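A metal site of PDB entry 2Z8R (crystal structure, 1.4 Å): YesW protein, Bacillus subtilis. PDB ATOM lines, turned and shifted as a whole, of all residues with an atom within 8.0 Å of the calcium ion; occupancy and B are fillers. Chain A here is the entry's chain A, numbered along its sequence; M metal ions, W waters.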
ATOM      1  N   GLY A  11     -20.859  20.755  37.305  1.00  0.00           N
ATOM      2  CA  GLY A  11     -21.567  20.818  36.031  1.00  0.00           C
ATOM      3  C   GLY A  11     -22.102  19.475  35.592  1.00  0.00           C
ATOM      4  O   GLY A  11     -22.263  19.222  34.414  1.00  0.00           O
ATOM      5  N   VAL A  13     -24.258  16.516  34.454  1.00  0.00           N
ATOM      6  CA  VAL A  13     -25.476  16.396  33.676  1.00  0.00           C
ATOM      7  C   VAL A  13     -25.667  14.926  33.326  1.00  0.00           C
ATOM      8  O   VAL A  13     -24.691  14.180  33.142  1.00  0.00           O
ATOM      9  CB  VAL A  13     -25.452  17.317  32.406  1.00  0.00           C
ATOM     10  CG1 VAL A  13     -24.448  16.812  31.378  1.00  0.00           C
ATOM     11  CG2 VAL A  13     -26.820  17.428  31.785  1.00  0.00           C
ATOM     12  N   SER A  24     -22.081  13.511  31.772  1.00  0.00           N
ATOM     13  CA  SER A  24     -20.814  14.226  31.578  1.00  0.00           C
ATOM     14  C   SER A  24     -20.657  15.311  32.640  1.00  0.00           C
ATOM     15  O   SER A  24     -21.638  15.705  33.277  1.00  0.00           O
ATOM     16  CB  SER A  24     -20.621  14.755  30.147  1.00  0.00           C
ATOM     17  OG  SER A  24     -21.323  15.962  29.904  1.00  0.00           O
ATOM     18  N   TRP A  25     -19.423  15.750  32.832  1.00  0.00           N
ATOM     19  CA  TRP A  25     -19.127  16.702  33.874  1.00  0.00           C
ATOM     20  C   TRP A  25     -17.846  17.473  33.574  1.00  0.00           C
ATOM     21  O   TRP A  25     -17.126  17.151  32.613  1.00  0.00           O
ATOM     22  CB  TRP A  25     -19.042  15.994  35.253  1.00  0.00           C
ATOM     23  CG  TRP A  25     -17.935  14.954  35.347  1.00  0.00           C
ATOM     24  CD1 TRP A  25     -16.667  15.151  35.785  1.00  0.00           C
ATOM     25  CD2 TRP A  25     -18.026  13.556  34.990  1.00  0.00           C
ATOM     26  NE1 TRP A  25     -15.950  13.967  35.730  1.00  0.00           N
ATOM     27  CE2 TRP A  25     -16.766  12.983  35.243  1.00  0.00           C
ATOM     28  CE3 TRP A  25     -19.045  12.746  34.461  1.00  0.00           C
ATOM     29  CZ2 TRP A  25     -16.492  11.623  35.004  1.00  0.00           C
ATOM     30  CZ3 TRP A  25     -18.770  11.395  34.227  1.00  0.00           C
ATOM     31  CH2 TRP A  25     -17.500  10.854  34.483  1.00  0.00           C
ATOM     32  N   ARG A  26     -17.567  18.483  34.387  1.00  0.00           N
ATOM     33  CA  ARG A  26     -16.446  19.369  34.166  1.00  0.00           C
ATOM     34  C   ARG A  26     -15.149  18.811  34.719  1.00  0.00           C
ATOM     35  O   ARG A  26     -15.123  18.192  35.783  1.00  0.00           O
ATOM     36  CB  ARG A  26     -16.696  20.712  34.849  1.00  0.00           C
ATOM     37  CG  ARG A  26     -17.816  21.525  34.272  1.00  0.00           C
ATOM     38  CD  ARG A  26     -18.181  22.657  35.202  1.00  0.00           C
ATOM     39  NE  ARG A  26     -19.091  23.614  34.584  1.00  0.00           N
ATOM     40  CZ  ARG A  26     -19.983  24.357  35.235  1.00  0.00           C
ATOM     41  NH1 ARG A  26     -20.147  24.235  36.543  1.00  0.00           N
ATOM     42  NH2 ARG A  26     -20.729  25.226  34.552  1.00  0.00           N
ATOM     43  N   TRP A 457     -17.824  22.873  19.148  1.00  0.00           N
ATOM     44  CA  TRP A 457     -17.349  21.537  19.509  1.00  0.00           C
ATOM     45  C   TRP A 457     -18.533  20.723  19.992  1.00  0.00           C
ATOM     46  O   TRP A 457     -19.031  20.951  21.095  1.00  0.00           O
ATOM     47  CB  TRP A 457     -16.234  21.587  20.565  1.00  0.00           C
ATOM     48  CG  TRP A 457     -14.964  22.176  20.014  1.00  0.00           C
ATOM     49  CD1 TRP A 457     -14.159  21.629  19.047  1.00  0.00           C
ATOM     50  CD2 TRP A 457     -14.365  23.443  20.348  1.00  0.00           C
ATOM     51  NE1 TRP A 457     -13.107  22.461  18.771  1.00  0.00           N
ATOM     52  CE2 TRP A 457     -13.206  23.585  19.548  1.00  0.00           C
ATOM     53  CE3 TRP A 457     -14.707  24.479  21.237  1.00  0.00           C
ATOM     54  CZ2 TRP A 457     -12.383  24.706  19.615  1.00  0.00           C
ATOM     55  CZ3 TRP A 457     -13.870  25.605  21.313  1.00  0.00           C
ATOM     56  CH2 TRP A 457     -12.723  25.698  20.501  1.00  0.00           C
ATOM     57  N   TRP A 458     -18.973  19.771  19.151  1.00  0.00           N
ATOM     58  CA  TRP A 458     -20.202  19.022  19.420  1.00  0.00           C
ATOM     59  C   TRP A 458     -19.990  17.521  19.537  1.00  0.00           C
ATOM     60  O   TRP A 458     -20.483  16.898  20.474  1.00  0.00           O
ATOM     61  CB  TRP A 458     -21.248  19.316  18.348  1.00  0.00           C
ATOM     62  CG  TRP A 458     -22.566  18.657  18.619  1.00  0.00           C
ATOM     63  CD1 TRP A 458     -23.120  17.616  17.926  1.00  0.00           C
ATOM     64  CD2 TRP A 458     -23.494  18.999  19.656  1.00  0.00           C
ATOM     65  NE1 TRP A 458     -24.350  17.284  18.480  1.00  0.00           N
ATOM     66  CE2 TRP A 458     -24.604  18.116  19.533  1.00  0.00           C
ATOM     67  CE3 TRP A 458     -23.502  19.968  20.675  1.00  0.00           C
ATOM     68  CZ2 TRP A 458     -25.710  18.183  20.400  1.00  0.00           C
ATOM     69  CZ3 TRP A 458     -24.610  20.026  21.537  1.00  0.00           C
ATOM     70  CH2 TRP A 458     -25.697  19.132  21.387  1.00  0.00           C
ATOM     71  N   ALA A 505     -22.299  27.892  24.360  1.00  0.00           N
ATOM     72  CA  ALA A 505     -21.282  27.926  25.405  1.00  0.00           C
ATOM     73  C   ALA A 505     -21.157  26.580  26.074  1.00  0.00           C
ATOM     74  O   ALA A 505     -22.154  25.879  26.224  1.00  0.00           O
ATOM     75  CB  ALA A 505     -21.609  28.992  26.466  1.00  0.00           C
ATOM     76  N   ASP A 506     -19.953  26.246  26.513  1.00  0.00           N
ATOM     77  CA  ASP A 506     -19.783  25.112  27.414  1.00  0.00           C
ATOM     78  C   ASP A 506     -20.274  25.520  28.816  1.00  0.00           C
ATOM     79  O   ASP A 506     -19.491  25.997  29.650  1.00  0.00           O
ATOM     80  CB  ASP A 506     -18.321  24.667  27.471  1.00  0.00           C
ATOM     81  CG  ASP A 506     -18.093  23.556  28.485  1.00  0.00           C
ATOM     82  OD1 ASP A 506     -19.076  22.885  28.869  1.00  0.00           O
ATOM     83  OD2 ASP A 506     -16.942  23.390  28.922  1.00  0.00           O
ATOM     84  N   LEU A 507     -21.583  25.313  29.034  1.00  0.00           N
ATOM     85  CA  LEU A 507     -22.308  25.774  30.225  1.00  0.00           C
ATOM     86  C   LEU A 507     -22.382  24.745  31.327  1.00  0.00           C
ATOM     87  O   LEU A 507     -22.568  25.070  32.494  1.00  0.00           O
ATOM     88  CB  LEU A 507     -23.745  26.158  29.854  1.00  0.00           C
ATOM     89  CG  LEU A 507     -23.929  27.418  28.997  1.00  0.00           C
ATOM     90  CD1 LEU A 507     -25.395  27.750  28.813  1.00  0.00           C
ATOM     91  CD2 LEU A 507     -23.179  28.570  29.634  1.00  0.00           C
ATOM     92  N   LEU A 508     -22.242  23.487  30.931  1.00  0.00           N
ATOM     93  CA  LEU A 508     -22.413  22.355  31.824  1.00  0.00           C
ATOM     94  C   LEU A 508     -21.782  21.123  31.163  1.00  0.00           C
ATOM     95  O   LEU A 508     -21.338  21.201  30.017  1.00  0.00           O
ATOM     96  CB  LEU A 508     -23.908  22.126  32.147  1.00  0.00           C
ATOM     97  CG  LEU A 508     -24.953  22.028  31.038  1.00  0.00           C
ATOM     98  CD1 LEU A 508     -24.871  20.721  30.304  1.00  0.00           C
ATOM     99  CD2 LEU A 508     -26.357  22.182  31.603  1.00  0.00           C
ATOM    100  N   GLY A 509     -21.725  20.019  31.890  1.00  0.00           N
ATOM    101  CA  GLY A 509     -21.080  18.780  31.427  1.00  0.00           C
ATOM    102  C   GLY A 509     -19.616  18.950  31.031  1.00  0.00           C
ATOM    103  O   GLY A 509     -18.929  19.851  31.530  1.00  0.00           O
ATOM    104  N   ASP A 510     -19.165  18.094  30.122  1.00  0.00           N
ATOM    105  CA  ASP A 510     -17.758  18.098  29.686  1.00  0.00           C
ATOM    106  C   ASP A 510     -17.473  19.214  28.691  1.00  0.00           C
ATOM    107  O   ASP A 510     -18.318  20.074  28.467  1.00  0.00           O
ATOM    108  CB  ASP A 510     -17.315  16.696  29.189  1.00  0.00           C
ATOM    109  CG  ASP A 510     -17.918  16.307  27.839  1.00  0.00           C
ATOM    110  OD1 ASP A 510     -18.435  17.170  27.115  1.00  0.00           O
ATOM    111  OD2 ASP A 510     -17.826  15.107  27.495  1.00  0.00           O
ATOM    112  N   TRP A 511     -16.287  19.183  28.097  1.00  0.00           N
ATOM    113  CA  TRP A 511     -15.798  20.303  27.298  1.00  0.00           C
ATOM    114  C   TRP A 511     -16.582  20.655  26.040  1.00  0.00           C
ATOM    115  O   TRP A 511     -16.371  21.735  25.504  1.00  0.00           O
ATOM    116  CB  TRP A 511     -14.332  20.077  26.934  1.00  0.00           C
ATOM    117  CG  TRP A 511     -14.105  18.879  26.053  1.00  0.00           C
ATOM    118  CD1 TRP A 511     -13.989  17.568  26.452  1.00  0.00           C
ATOM    119  CD2 TRP A 511     -13.976  18.868  24.618  1.00  0.00           C
ATOM    120  NE1 TRP A 511     -13.771  16.750  25.360  1.00  0.00           N
ATOM    121  CE2 TRP A 511     -13.765  17.518  24.226  1.00  0.00           C
ATOM    122  CE3 TRP A 511     -13.984  19.872  23.642  1.00  0.00           C
ATOM    123  CZ2 TRP A 511     -13.595  17.154  22.883  1.00  0.00           C
ATOM    124  CZ3 TRP A 511     -13.811  19.503  22.308  1.00  0.00           C
ATOM    125  CH2 TRP A 511     -13.601  18.161  21.945  1.00  0.00           C
ATOM    126  N   ARG A 512     -17.441  19.778  25.534  1.00  0.00           N
ATOM    127  CA  ARG A 512     -18.228  20.151  24.363  1.00  0.00           C
ATOM    128  C   ARG A 512     -19.167  21.315  24.696  1.00  0.00           C
ATOM    129  O   ARG A 512     -19.497  21.568  25.861  1.00  0.00           O
ATOM    130  CB  ARG A 512     -18.998  18.969  23.789  1.00  0.00           C
ATOM    131  CG  ARG A 512     -18.183  18.116  22.832  1.00  0.00           C
ATOM    132  CD  ARG A 512     -17.194  17.174  23.529  1.00  0.00           C
ATOM    133  NE  ARG A 512     -17.832  16.225  24.448  1.00  0.00           N
ATOM    134  CZ  ARG A 512     -18.414  15.087  24.062  1.00  0.00           C
ATOM    135  NH1 ARG A 512     -18.491  14.767  22.777  1.00  0.00           N
ATOM    136  NH2 ARG A 512     -18.957  14.289  24.975  1.00  0.00           N
ATOM    137  N   GLU A 513     -19.569  22.043  23.666  1.00  0.00           N
ATOM    138  CA  GLU A 513     -20.367  23.228  23.886  1.00  0.00           C
ATOM    139  C   GLU A 513     -21.860  22.917  23.793  1.00  0.00           C
ATOM    140  O   GLU A 513     -22.306  22.173  22.907  1.00  0.00           O
ATOM    141  CB  GLU A 513     -19.996  24.296  22.855  1.00  0.00           C
ATOM    142  CG  GLU A 513     -18.524  24.656  22.863  1.00  0.00           C
ATOM    143  CD  GLU A 513     -18.177  25.663  21.780  1.00  0.00           C
ATOM    144  OE1 GLU A 513     -17.808  25.238  20.670  1.00  0.00           O
ATOM    145  OE2 GLU A 513     -18.321  26.884  22.034  1.00  0.00           O
ATOM    146  N   GLU A 514     -22.612  23.510  24.707  1.00  0.00           N
ATOM    147  CA  GLU A 514     -24.068  23.470  24.676  1.00  0.00           C
ATOM    148  C   GLU A 514     -24.597  24.533  23.734  1.00  0.00           C
ATOM    149  O   GLU A 514     -23.921  25.535  23.466  1.00  0.00           O
ATOM    150  CB  GLU A 514     -24.645  23.695  26.075  1.00  0.00           C
ATOM    151  CG  GLU A 514     -24.503  22.507  27.039  1.00  0.00           C
ATOM    152  CD  GLU A 514     -23.055  22.068  27.276  1.00  0.00           C
ATOM    153  OE1 GLU A 514     -22.229  22.883  27.734  1.00  0.00           O
ATOM    154  OE2 GLU A 514     -22.715  20.880  27.043  1.00  0.00           O
ATOM    155  N   VAL A 515     -25.818  24.315  23.241  1.00  0.00           N
ATOM    156  CA  VAL A 515     -26.527  25.316  22.475  1.00  0.00           C
ATOM    157  C   VAL A 515     -27.828  25.632  23.184  1.00  0.00           C
ATOM    158  O   VAL A 515     -28.561  24.713  23.608  1.00  0.00           O
ATOM    159  CB  VAL A 515     -26.885  24.855  21.052  1.00  0.00           C
ATOM    160  CG1 VAL A 515     -27.364  26.049  20.218  1.00  0.00           C
ATOM    161  CG2 VAL A 515     -25.685  24.199  20.362  1.00  0.00           C
ATOM    162  N   TYR A 528     -29.408  22.316  24.661  1.00  0.00           N
ATOM    163  CA  TYR A 528     -28.972  21.031  24.102  1.00  0.00           C
ATOM    164  C   TYR A 528     -27.551  20.748  24.564  1.00  0.00           C
ATOM    165  O   TYR A 528     -26.663  21.624  24.497  1.00  0.00           O
ATOM    166  CB  TYR A 528     -29.004  21.069  22.573  1.00  0.00           C
ATOM    167  CG  TYR A 528     -30.390  21.034  21.969  1.00  0.00           C
ATOM    168  CD1 TYR A 528     -30.881  19.872  21.377  1.00  0.00           C
ATOM    169  CD2 TYR A 528     -31.194  22.165  21.976  1.00  0.00           C
ATOM    170  CE1 TYR A 528     -32.157  19.835  20.817  1.00  0.00           C
ATOM    171  CE2 TYR A 528     -32.484  22.145  21.407  1.00  0.00           C
ATOM    172  CZ  TYR A 528     -32.947  20.979  20.837  1.00  0.00           C
ATOM    173  OH  TYR A 528     -34.219  20.968  20.291  1.00  0.00           O
ATOM    174  N   THR A 529     -27.312  19.538  25.063  1.00  0.00           N
ATOM    175  CA  THR A 529     -25.973  19.113  25.448  1.00  0.00           C
ATOM    176  C   THR A 529     -25.687  17.816  24.693  1.00  0.00           C
ATOM    177  O   THR A 529     -26.593  16.989  24.527  1.00  0.00           O
ATOM    178  CB  THR A 529     -25.814  18.941  26.984  1.00  0.00           C
ATOM    179  OG1 THR A 529     -24.432  18.829  27.331  1.00  0.00           O
ATOM    180  CG2 THR A 529     -26.551  17.698  27.497  1.00  0.00           C
ATOM    181  N   THR A 530     -24.464  17.658  24.217  1.00  0.00           N
ATOM    182  CA  THR A 530     -24.159  16.477  23.413  1.00  0.00           C
ATOM    183  C   THR A 530     -24.186  15.193  24.236  1.00  0.00           C
ATOM    184  O   THR A 530     -23.829  15.211  25.421  1.00  0.00           O
ATOM    185  CB  THR A 530     -22.802  16.617  22.698  1.00  0.00           C
ATOM    186  OG1 THR A 530     -22.710  15.629  21.673  1.00  0.00           O
ATOM    187  CG2 THR A 530     -21.631  16.477  23.668  1.00  0.00           C
ATOM    188  N   THR A 540     -12.819  22.754  31.503  1.00  0.00           N
ATOM    189  CA  THR A 540     -14.059  23.403  31.105  1.00  0.00           C
ATOM    190  C   THR A 540     -13.701  24.702  30.388  1.00  0.00           C
ATOM    191  O   THR A 540     -12.816  25.454  30.822  1.00  0.00           O
ATOM    192  CB  THR A 540     -15.037  23.626  32.286  1.00  0.00           C
ATOM    193  OG1 THR A 540     -16.194  24.315  31.795  1.00  0.00           O
ATOM    194  CG2 THR A 540     -14.413  24.452  33.399  1.00  0.00           C
ATOM    195  N   LEU A 541     -14.369  24.942  29.265  1.00  0.00           N
ATOM    196  CA  LEU A 541     -13.962  26.067  28.413  1.00  0.00           C
ATOM    197  C   LEU A 541     -14.154  27.408  29.110  1.00  0.00           C
ATOM    198  O   LEU A 541     -13.481  28.382  28.767  1.00  0.00           O
ATOM    199  CB  LEU A 541     -14.662  26.007  27.050  1.00  0.00           C
ATOM    200  CG  LEU A 541     -14.519  24.661  26.332  1.00  0.00           C
ATOM    201  CD1 LEU A 541     -15.179  24.751  24.958  1.00  0.00           C
ATOM    202  CD2 LEU A 541     -13.057  24.205  26.200  1.00  0.00           C
ATOM    203  N   TYR A 547     -11.805  32.057  25.855  1.00  0.00           N
ATOM    204  CA  TYR A 547     -13.145  31.517  25.642  1.00  0.00           C
ATOM    205  C   TYR A 547     -14.165  32.189  26.556  1.00  0.00           C
ATOM    206  O   TYR A 547     -15.249  32.583  26.107  1.00  0.00           O
ATOM    207  CB  TYR A 547     -13.152  29.994  25.828  1.00  0.00           C
ATOM    208  CG  TYR A 547     -14.467  29.351  25.483  1.00  0.00           C
ATOM    209  CD1 TYR A 547     -14.665  28.764  24.232  1.00  0.00           C
ATOM    210  CD2 TYR A 547     -15.535  29.345  26.391  1.00  0.00           C
ATOM    211  CE1 TYR A 547     -15.883  28.169  23.904  1.00  0.00           C
ATOM    212  CE2 TYR A 547     -16.753  28.771  26.064  1.00  0.00           C
ATOM    213  CZ  TYR A 547     -16.923  28.171  24.831  1.00  0.00           C
ATOM    214  OH  TYR A 547     -18.141  27.591  24.537  1.00  0.00           O
HETATM  215 CA    CA M   1     -20.400  21.081  27.923  1.00  0.00          CA
HETATM  216  O   HOH W   1     -20.663  18.715  27.361  1.00  0.00           O
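The calcium ion is bound by the backbone carbonyl oxygen (O) of Leu 508, the backbone carbonyl oxygen (O) of Arg 512, the backbone carbonyl oxygen (O) of Asp 510, the side-chain carboxylate (OD1) of Asp 506, water W1, the side-chain carboxylate (OE2) of Glu 514 and the side-chain carboxylate (OE1) of Glu 514.
The calcium ion has seven donor atoms within binding distance.
The backbone NH (N) of Asp 510 sits close to the backbone carbonyl oxygen (O) of Trp 25, 3.4 Å away.
The side-chain hydroxyl (OG1) of Thr 540 lies within hydrogen-bond range of the side-chain carboxylate (OD2) of Asp 506 (3.1 Å).
The backbone NH (N) of Leu 541 lies within hydrogen-bond range of the side-chain carboxylate (OD2) of Asp 506 (3.0 Å).
N of Asp 506 sits at hydrogen-bond distance from OH of Tyr 547 (3.0 Å).
The side-chain carboxylate (OE1) of Glu 514 sits close to the backbone NH (N) of Leu 507 (2.8 Å).
The backbone NH (N) of Glu 514 sits at hydrogen-bond distance from the backbone carbonyl oxygen (O) of Ala 505, 2.9 Å away.
The backbone NH (N) of Arg 26 lies close to the backbone carbonyl oxygen (O) of Gly 509.
N of Gly 509 lies within hydrogen-bond range of O of Gly 11, 2.7 Å away.
C of Gly 509 touches the calcium ion (3.8 Å).
Six residues have an atom within 4 Å of the calcium ion: Asp 506, Leu 508, Gly 509, Asp 510, Arg 512 and Glu 514.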
